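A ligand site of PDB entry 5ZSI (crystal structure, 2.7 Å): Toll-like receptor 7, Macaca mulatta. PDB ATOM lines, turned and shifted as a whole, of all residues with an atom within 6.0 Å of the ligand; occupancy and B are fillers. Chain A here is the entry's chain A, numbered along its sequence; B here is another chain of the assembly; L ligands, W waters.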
ATOM      1  N   THR A 510       4.709  -2.086 -20.855  1.00  0.00           N
ATOM      2  CA  THR A 510       4.035  -3.308 -21.304  1.00  0.00           C
ATOM      3  C   THR A 510       4.917  -4.487 -20.904  1.00  0.00           C
ATOM      4  O   THR A 510       6.048  -4.601 -21.381  1.00  0.00           O
ATOM      5  CB  THR A 510       3.803  -3.342 -22.813  1.00  0.00           C
ATOM      6  OG1 THR A 510       5.026  -3.646 -23.472  1.00  0.00           O
ATOM      7  CG2 THR A 510       3.302  -2.021 -23.362  1.00  0.00           C
ATOM      8  N   ASP A 533       0.521  -1.832 -18.405  1.00  0.00           N
ATOM      9  CA  ASP A 533      -0.148  -1.877 -19.705  1.00  0.00           C
ATOM     10  C   ASP A 533      -0.208  -3.327 -20.157  1.00  0.00           C
ATOM     11  O   ASP A 533       0.798  -3.879 -20.616  1.00  0.00           O
ATOM     12  CB  ASP A 533       0.597  -1.019 -20.715  1.00  0.00           C
ATOM     13  CG  ASP A 533      -0.106  -0.968 -22.044  1.00  0.00           C
ATOM     14  OD1 ASP A 533      -1.203  -1.547 -22.206  1.00  0.00           O
ATOM     15  OD2 ASP A 533       0.488  -0.365 -22.951  1.00  0.00           O
ATOM     16  N   LEU A 534      -1.391  -3.931 -20.047  1.00  0.00           N
ATOM     17  CA  LEU A 534      -1.623  -5.324 -20.401  1.00  0.00           C
ATOM     18  C   LEU A 534      -1.785  -5.486 -21.913  1.00  0.00           C
ATOM     19  O   LEU A 534      -2.788  -5.996 -22.413  1.00  0.00           O
ATOM     20  CB  LEU A 534      -2.855  -5.842 -19.668  1.00  0.00           C
ATOM     21  CG  LEU A 534      -2.637  -6.322 -18.248  1.00  0.00           C
ATOM     22  CD1 LEU A 534      -3.981  -6.689 -17.639  1.00  0.00           C
ATOM     23  CD2 LEU A 534      -1.697  -7.527 -18.258  1.00  0.00           C
ATOM     24  N   LEU A 535      -0.771  -5.041 -22.659  1.00  0.00           N
ATOM     25  CA  LEU A 535      -0.800  -5.271 -24.097  1.00  0.00           C
ATOM     26  C   LEU A 535      -0.612  -6.743 -24.431  1.00  0.00           C
ATOM     27  O   LEU A 535      -1.191  -7.235 -25.400  1.00  0.00           O
ATOM     28  CB  LEU A 535       0.266  -4.450 -24.809  1.00  0.00           C
ATOM     29  CG  LEU A 535       0.375  -4.734 -26.305  1.00  0.00           C
ATOM     30  CD1 LEU A 535      -0.862  -4.194 -26.937  1.00  0.00           C
ATOM     31  CD2 LEU A 535       1.571  -4.070 -26.917  1.00  0.00           C
ATOM     32  N   TYR A 557      -3.831   2.934 -18.048  1.00  0.00           N
ATOM     33  CA  TYR A 557      -4.104   2.476 -19.400  1.00  0.00           C
ATOM     34  C   TYR A 557      -5.526   1.945 -19.557  1.00  0.00           C
ATOM     35  O   TYR A 557      -6.065   1.975 -20.667  1.00  0.00           O
ATOM     36  CB  TYR A 557      -3.061   1.422 -19.817  1.00  0.00           C
ATOM     37  CG  TYR A 557      -1.722   2.045 -20.149  1.00  0.00           C
ATOM     38  CD1 TYR A 557      -1.510   2.709 -21.337  1.00  0.00           C
ATOM     39  CD2 TYR A 557      -0.674   1.988 -19.241  1.00  0.00           C
ATOM     40  CE1 TYR A 557      -0.291   3.295 -21.633  1.00  0.00           C
ATOM     41  CE2 TYR A 557       0.549   2.570 -19.529  1.00  0.00           C
ATOM     42  CZ  TYR A 557       0.729   3.228 -20.718  1.00  0.00           C
ATOM     43  OH  TYR A 557       1.946   3.790 -20.977  1.00  0.00           O
ATOM     44  N   GLU A 561      -9.658   5.269 -24.154  1.00  0.00           N
ATOM     45  CA  GLU A 561     -10.366   4.812 -25.315  1.00  0.00           C
ATOM     46  C   GLU A 561      -9.634   3.754 -26.131  1.00  0.00           C
ATOM     47  O   GLU A 561      -8.518   3.976 -26.553  1.00  0.00           O
ATOM     48  CB  GLU A 561     -10.512   6.040 -26.202  1.00  0.00           C
ATOM     49  CG  GLU A 561     -11.817   6.664 -26.462  1.00  0.00           C
ATOM     50  CD  GLU A 561     -11.496   7.675 -27.438  1.00  0.00           C
ATOM     51  OE1 GLU A 561     -11.231   8.807 -27.044  1.00  0.00           O
ATOM     52  OE2 GLU A 561     -11.310   7.346 -28.613  1.00  0.00           O
ATOM     53  N   GLY A 562     -10.254   2.601 -26.310  1.00  0.00           N
ATOM     54  CA  GLY A 562      -9.954   1.835 -27.517  1.00  0.00           C
ATOM     55  C   GLY A 562      -8.644   1.086 -27.512  1.00  0.00           C
ATOM     56  O   GLY A 562      -8.346   0.371 -28.480  1.00  0.00           O
ATOM     57  N   ILE A 563      -7.845   1.279 -26.474  1.00  0.00           N
ATOM     58  CA  ILE A 563      -6.571   0.602 -26.291  1.00  0.00           C
ATOM     59  C   ILE A 563      -6.818  -0.865 -25.953  1.00  0.00           C
ATOM     60  O   ILE A 563      -7.808  -1.232 -25.300  1.00  0.00           O
ATOM     61  CB  ILE A 563      -5.823   1.379 -25.183  1.00  0.00           C
ATOM     62  CG1 ILE A 563      -5.019   2.537 -25.775  1.00  0.00           C
ATOM     63  CG2 ILE A 563      -4.887   0.545 -24.362  1.00  0.00           C
ATOM     64  CD1 ILE A 563      -5.682   3.349 -26.809  1.00  0.00           C
ATOM     65  N   THR A 564      -5.894  -1.718 -26.403  1.00  0.00           N
ATOM     66  CA  THR A 564      -5.969  -3.155 -26.128  1.00  0.00           C
ATOM     67  C   THR A 564      -5.682  -3.436 -24.657  1.00  0.00           C
ATOM     68  O   THR A 564      -4.792  -2.828 -24.064  1.00  0.00           O
ATOM     69  CB  THR A 564      -4.945  -3.914 -26.992  1.00  0.00           C
ATOM     70  OG1 THR A 564      -5.332  -3.918 -28.375  1.00  0.00           O
ATOM     71  CG2 THR A 564      -4.828  -5.342 -26.555  1.00  0.00           C
ATOM     72  N   HIS A 565      -6.421  -4.394 -24.072  1.00  0.00           N
ATOM     73  CA  HIS A 565      -6.213  -4.848 -22.695  1.00  0.00           C
ATOM     74  C   HIS A 565      -6.359  -6.365 -22.640  1.00  0.00           C
ATOM     75  O   HIS A 565      -7.435  -6.895 -22.945  1.00  0.00           O
ATOM     76  CB  HIS A 565      -7.224  -4.246 -21.714  1.00  0.00           C
ATOM     77  CG  HIS A 565      -7.338  -2.752 -21.784  1.00  0.00           C
ATOM     78  ND1 HIS A 565      -8.489  -2.118 -22.196  1.00  0.00           N
ATOM     79  CD2 HIS A 565      -6.476  -1.768 -21.428  1.00  0.00           C
ATOM     80  CE1 HIS A 565      -8.322  -0.813 -22.141  1.00  0.00           C
ATOM     81  NE2 HIS A 565      -7.113  -0.571 -21.662  1.00  0.00           N
ATOM     82  N   TYR B 242     -12.012  -3.992 -34.213  1.00  0.00           N
ATOM     83  CA  TYR B 242     -11.023  -4.332 -33.185  1.00  0.00           C
ATOM     84  C   TYR B 242     -11.158  -3.401 -31.990  1.00  0.00           C
ATOM     85  O   TYR B 242     -11.179  -2.175 -32.138  1.00  0.00           O
ATOM     86  CB  TYR B 242      -9.620  -4.236 -33.748  1.00  0.00           C
ATOM     87  CG  TYR B 242      -8.518  -4.714 -32.823  1.00  0.00           C
ATOM     88  CD1 TYR B 242      -8.439  -6.041 -32.425  1.00  0.00           C
ATOM     89  CD2 TYR B 242      -7.514  -3.848 -32.388  1.00  0.00           C
ATOM     90  CE1 TYR B 242      -7.405  -6.493 -31.602  1.00  0.00           C
ATOM     91  CE2 TYR B 242      -6.488  -4.291 -31.581  1.00  0.00           C
ATOM     92  CZ  TYR B 242      -6.433  -5.612 -31.181  1.00  0.00           C
ATOM     93  OH  TYR B 242      -5.403  -6.060 -30.366  1.00  0.00           O
ATOM     94  N   ASN B 243     -11.264  -3.996 -30.801  1.00  0.00           N
ATOM     95  CA  ASN B 243     -11.447  -3.259 -29.566  1.00  0.00           C
ATOM     96  C   ASN B 243     -12.721  -2.422 -29.602  1.00  0.00           C
ATOM     97  O   ASN B 243     -12.782  -1.362 -28.998  1.00  0.00           O
ATOM     98  CB  ASN B 243     -10.257  -2.364 -29.264  1.00  0.00           C
ATOM     99  CG  ASN B 243      -9.024  -3.138 -28.868  1.00  0.00           C
ATOM    100  OD1 ASN B 243      -9.106  -4.282 -28.394  1.00  0.00           O
ATOM    101  ND2 ASN B 243      -7.862  -2.516 -29.033  1.00  0.00           N
ATOM    102  N   PHE B 327      -7.081   6.870 -35.381  1.00  0.00           N
ATOM    103  CA  PHE B 327      -7.275   5.434 -35.223  1.00  0.00           C
ATOM    104  C   PHE B 327      -7.317   4.714 -36.579  1.00  0.00           C
ATOM    105  O   PHE B 327      -8.246   3.960 -36.901  1.00  0.00           O
ATOM    106  CB  PHE B 327      -8.518   5.165 -34.375  1.00  0.00           C
ATOM    107  CG  PHE B 327      -8.359   5.618 -32.961  1.00  0.00           C
ATOM    108  CD1 PHE B 327      -7.546   4.907 -32.090  1.00  0.00           C
ATOM    109  CD2 PHE B 327      -8.978   6.773 -32.502  1.00  0.00           C
ATOM    110  CE1 PHE B 327      -7.360   5.323 -30.796  1.00  0.00           C
ATOM    111  CE2 PHE B 327      -8.790   7.213 -31.207  1.00  0.00           C
ATOM    112  CZ  PHE B 327      -7.980   6.473 -30.350  1.00  0.00           C
ATOM    113  N   PHE B 329      -4.294   3.061 -37.282  1.00  0.00           N
ATOM    114  CA  PHE B 329      -3.094   2.278 -37.072  1.00  0.00           C
ATOM    115  C   PHE B 329      -3.264   0.895 -37.683  1.00  0.00           C
ATOM    116  O   PHE B 329      -4.395   0.395 -37.811  1.00  0.00           O
ATOM    117  CB  PHE B 329      -2.805   2.153 -35.578  1.00  0.00           C
ATOM    118  CG  PHE B 329      -3.810   1.303 -34.836  1.00  0.00           C
ATOM    119  CD1 PHE B 329      -5.020   1.841 -34.424  1.00  0.00           C
ATOM    120  CD2 PHE B 329      -3.540  -0.020 -34.549  1.00  0.00           C
ATOM    121  CE1 PHE B 329      -5.951   1.072 -33.747  1.00  0.00           C
ATOM    122  CE2 PHE B 329      -4.456  -0.798 -33.871  1.00  0.00           C
ATOM    123  CZ  PHE B 329      -5.669  -0.264 -33.473  1.00  0.00           C
ATOM    124  N   VAL B 333       1.366  -3.559 -35.258  1.00  0.00           N
ATOM    125  CA  VAL B 333       2.531  -2.841 -35.740  1.00  0.00           C
ATOM    126  C   VAL B 333       2.804  -1.618 -34.883  1.00  0.00           C
ATOM    127  O   VAL B 333       1.874  -0.895 -34.477  1.00  0.00           O
ATOM    128  CB  VAL B 333       2.311  -2.442 -37.204  1.00  0.00           C
ATOM    129  CG1 VAL B 333       3.449  -1.583 -37.671  1.00  0.00           C
ATOM    130  CG2 VAL B 333       2.211  -3.682 -38.015  1.00  0.00           C
ATOM    131  N   TYR B 334       4.081  -1.376 -34.607  1.00  0.00           N
ATOM    132  CA  TYR B 334       4.522  -0.205 -33.856  1.00  0.00           C
ATOM    133  C   TYR B 334       5.492   0.595 -34.719  1.00  0.00           C
ATOM    134  O   TYR B 334       6.709   0.511 -34.519  1.00  0.00           O
ATOM    135  CB  TYR B 334       5.176  -0.670 -32.556  1.00  0.00           C
ATOM    136  CG  TYR B 334       5.317   0.376 -31.488  1.00  0.00           C
ATOM    137  CD1 TYR B 334       4.897   1.681 -31.703  1.00  0.00           C
ATOM    138  CD2 TYR B 334       5.848   0.047 -30.254  1.00  0.00           C
ATOM    139  CE1 TYR B 334       5.030   2.647 -30.699  1.00  0.00           C
ATOM    140  CE2 TYR B 334       5.970   0.985 -29.248  1.00  0.00           C
ATOM    141  CZ  TYR B 334       5.561   2.285 -29.470  1.00  0.00           C
ATOM    142  OH  TYR B 334       5.709   3.221 -28.453  1.00  0.00           O
ATOM    143  N   GLY B 357      -4.144   7.790 -32.484  1.00  0.00           N
ATOM    144  CA  GLY B 357      -4.149   6.368 -32.812  1.00  0.00           C
ATOM    145  C   GLY B 357      -3.540   5.998 -34.156  1.00  0.00           C
ATOM    146  O   GLY B 357      -4.063   5.111 -34.849  1.00  0.00           O
ATOM    147  N   VAL B 359      -0.121   5.498 -33.925  1.00  0.00           N
ATOM    148  CA  VAL B 359       0.813   4.656 -33.168  1.00  0.00           C
ATOM    149  C   VAL B 359       2.205   4.700 -33.766  1.00  0.00           C
ATOM    150  O   VAL B 359       2.463   4.112 -34.832  1.00  0.00           O
ATOM    151  CB  VAL B 359       0.289   3.215 -33.057  1.00  0.00           C
ATOM    152  CG1 VAL B 359       1.209   2.390 -32.199  1.00  0.00           C
ATOM    153  CG2 VAL B 359      -1.108   3.229 -32.437  1.00  0.00           C
ATOM    154  N   THR B 384      -2.890   9.767 -27.850  1.00  0.00           N
ATOM    155  CA  THR B 384      -3.079   8.307 -27.879  1.00  0.00           C
ATOM    156  C   THR B 384      -2.345   7.710 -29.073  1.00  0.00           C
ATOM    157  O   THR B 384      -2.926   7.079 -29.957  1.00  0.00           O
ATOM    158  CB  THR B 384      -4.559   7.942 -27.882  1.00  0.00           C
ATOM    159  OG1 THR B 384      -5.245   8.672 -26.860  1.00  0.00           O
ATOM    160  CG2 THR B 384      -4.768   6.454 -27.648  1.00  0.00           C
ATOM    161  N   PHE B 386       1.129   6.523 -28.319  1.00  0.00           N
ATOM    162  CA  PHE B 386       2.214   5.774 -27.693  1.00  0.00           C
ATOM    163  C   PHE B 386       3.574   6.318 -28.102  1.00  0.00           C
ATOM    164  O   PHE B 386       4.556   5.577 -28.162  1.00  0.00           O
ATOM    165  CB  PHE B 386       2.083   4.275 -27.980  1.00  0.00           C
ATOM    166  CG  PHE B 386       0.798   3.672 -27.453  1.00  0.00           C
ATOM    167  CD1 PHE B 386       0.753   3.146 -26.181  1.00  0.00           C
ATOM    168  CD2 PHE B 386      -0.368   3.679 -28.211  1.00  0.00           C
ATOM    169  CE1 PHE B 386      -0.435   2.610 -25.688  1.00  0.00           C
ATOM    170  CE2 PHE B 386      -1.556   3.142 -27.717  1.00  0.00           C
ATOM    171  CZ  PHE B 386      -1.575   2.603 -26.453  1.00  0.00           C
ATOM    172  N   LYS B 410       3.577   8.281 -24.333  1.00  0.00           N
ATOM    173  CA  LYS B 410       4.598   7.682 -23.474  1.00  0.00           C
ATOM    174  C   LYS B 410       5.854   8.549 -23.425  1.00  0.00           C
ATOM    175  O   LYS B 410       6.961   8.039 -23.257  1.00  0.00           O
ATOM    176  CB  LYS B 410       4.950   6.277 -23.970  1.00  0.00           C
ATOM    177  CG  LYS B 410       4.012   5.134 -23.578  1.00  0.00           C
ATOM    178  CD  LYS B 410       4.706   3.772 -23.878  1.00  0.00           C
ATOM    179  CE  LYS B 410       5.208   3.109 -22.566  1.00  0.00           C
ATOM    180  NZ  LYS B 410       6.115   1.907 -22.743  1.00  0.00           N
ATOM    181  N   PHE B 444     -14.502   5.717 -29.872  1.00  0.00           N
ATOM    182  CA  PHE B 444     -14.946   4.336 -29.790  1.00  0.00           C
ATOM    183  C   PHE B 444     -16.402   4.184 -29.344  1.00  0.00           C
ATOM    184  O   PHE B 444     -16.964   3.100 -29.538  1.00  0.00           O
ATOM    185  CB  PHE B 444     -13.997   3.505 -28.912  1.00  0.00           C
ATOM    186  CG  PHE B 444     -12.762   3.053 -29.657  1.00  0.00           C
ATOM    187  CD1 PHE B 444     -12.700   1.789 -30.262  1.00  0.00           C
ATOM    188  CD2 PHE B 444     -11.688   3.903 -29.829  1.00  0.00           C
ATOM    189  CE1 PHE B 444     -11.553   1.372 -30.996  1.00  0.00           C
ATOM    190  CE2 PHE B 444     -10.555   3.507 -30.545  1.00  0.00           C
ATOM    191  CZ  PHE B 444     -10.489   2.238 -31.142  1.00  0.00           C
HETATM  192  N1  LIG L   1      -2.067  -1.136 -24.655  1.00  0.00           N
HETATM  193  C1  LIG L   1      -1.308  -0.823 -25.734  1.00  0.00           C
HETATM  194  C2  LIG L   1      -1.923  -0.806 -27.074  1.00  0.00           C
HETATM  195  N2  LIG L   1      -3.147  -1.030 -27.586  1.00  0.00           N
HETATM  196  C3  LIG L   1      -3.056  -0.847 -28.930  1.00  0.00           C
HETATM  197  C4  LIG L   1      -4.210  -0.971 -29.875  1.00  0.00           C
HETATM  198  O1  LIG L   1      -4.885   0.289 -29.824  1.00  0.00           O
HETATM  199  C5  LIG L   1      -4.081   1.356 -30.294  1.00  0.00           C
HETATM  200  C6  LIG L   1      -4.990   2.468 -30.730  1.00  0.00           C
HETATM  201  N3  LIG L   1      -1.806  -0.508 -29.302  1.00  0.00           N
HETATM  202  C7  LIG L   1      -1.063  -0.475 -28.203  1.00  0.00           C
HETATM  203  C8  LIG L   1       0.282  -0.196 -28.036  1.00  0.00           C
HETATM  204  C9  LIG L   1       1.141   0.126 -29.096  1.00  0.00           C
HETATM  205  C10 LIG L   1       2.490   0.405 -28.833  1.00  0.00           C
HETATM  206  C11 LIG L   1       2.997   0.355 -27.534  1.00  0.00           C
HETATM  207  C12 LIG L   1       2.176   0.030 -26.458  1.00  0.00           C
HETATM  208  C13 LIG L   1       0.821  -0.244 -26.654  1.00  0.00           C
HETATM  209  N4  LIG L   1       0.017  -0.546 -25.608  1.00  0.00           N
HETATM  210  O   HOH W   1      -1.035  -0.945 -32.084  1.00  0.00           O
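N of Thr 564 is in hydrogen-bond range of N2 of the ligand (3.1 Å). OD1 of Asp 533 lies within hydrogen-bond range of N1 of the ligand (2.6 Å). A nitrogen (N1) of the ligand is in hydrogen-bond range of the backbone carbonyl oxygen (O) of Thr 564, at 3.3 Å.
The side-chain hydroxyl (OG1) of Thr 564 is in hydrogen-bond range of the side-chain hydroxyl (OH) of Tyr 242 of chain B (2.9 Å). OG1 of Thr 564 lies within hydrogen-bond range of ND2 of Asn 243 of chain B. N of Phe 329 of chain B is in hydrogen-bond range of O of Gly 357 of chain B (3.2 Å). The backbone carbonyl oxygen of Phe 386 of chain B lies within hydrogen-bond range of the side-chain hydroxyl of Tyr 334 of chain B, 2.6 Å away. The side-chain amide nitrogen (ND2) of Asn 243 of chain B sits at hydrogen-bond distance from the backbone carbonyl oxygen (O) of Gly 562 (3.0 Å). O of Ile 563 lies close to ND1 of His 565 (3.3 Å).
Thr 510 touches the ligand. CD1 of Leu 535 touches C2 of the ligand (3.6 Å). O of Gly 562 touches O1 of the ligand, at 3.7 Å. Ile 563 touches the ligand (CG2 to N1, 3.3 Å). CE1 of Phe 327 of chain B touches C6 of the ligand, 3.7 Å away. CE1 of Phe 329 of chain B touches C6 of the ligand, at 3.5 Å. Tyr 334 of chain B touches the ligand (CE2 to C11, 3.5 Å). CG1 of Val 359 of chain B touches C9 of the ligand, at 3.8 Å. CE1 of Phe 386 of chain B touches N4 of the ligand (3.2 Å). Hydrophobic or aromatic side chains within 4 Å of the ligand: Leu 535, Ile 563, Phe 327 of chain B, Phe 329 of chain B, Tyr 334 of chain B, Val 359 of chain B and Phe 386 of chain B. The nearest printed residue that does not touch the ligand is Asn 243 of chain B (4.1 Å).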
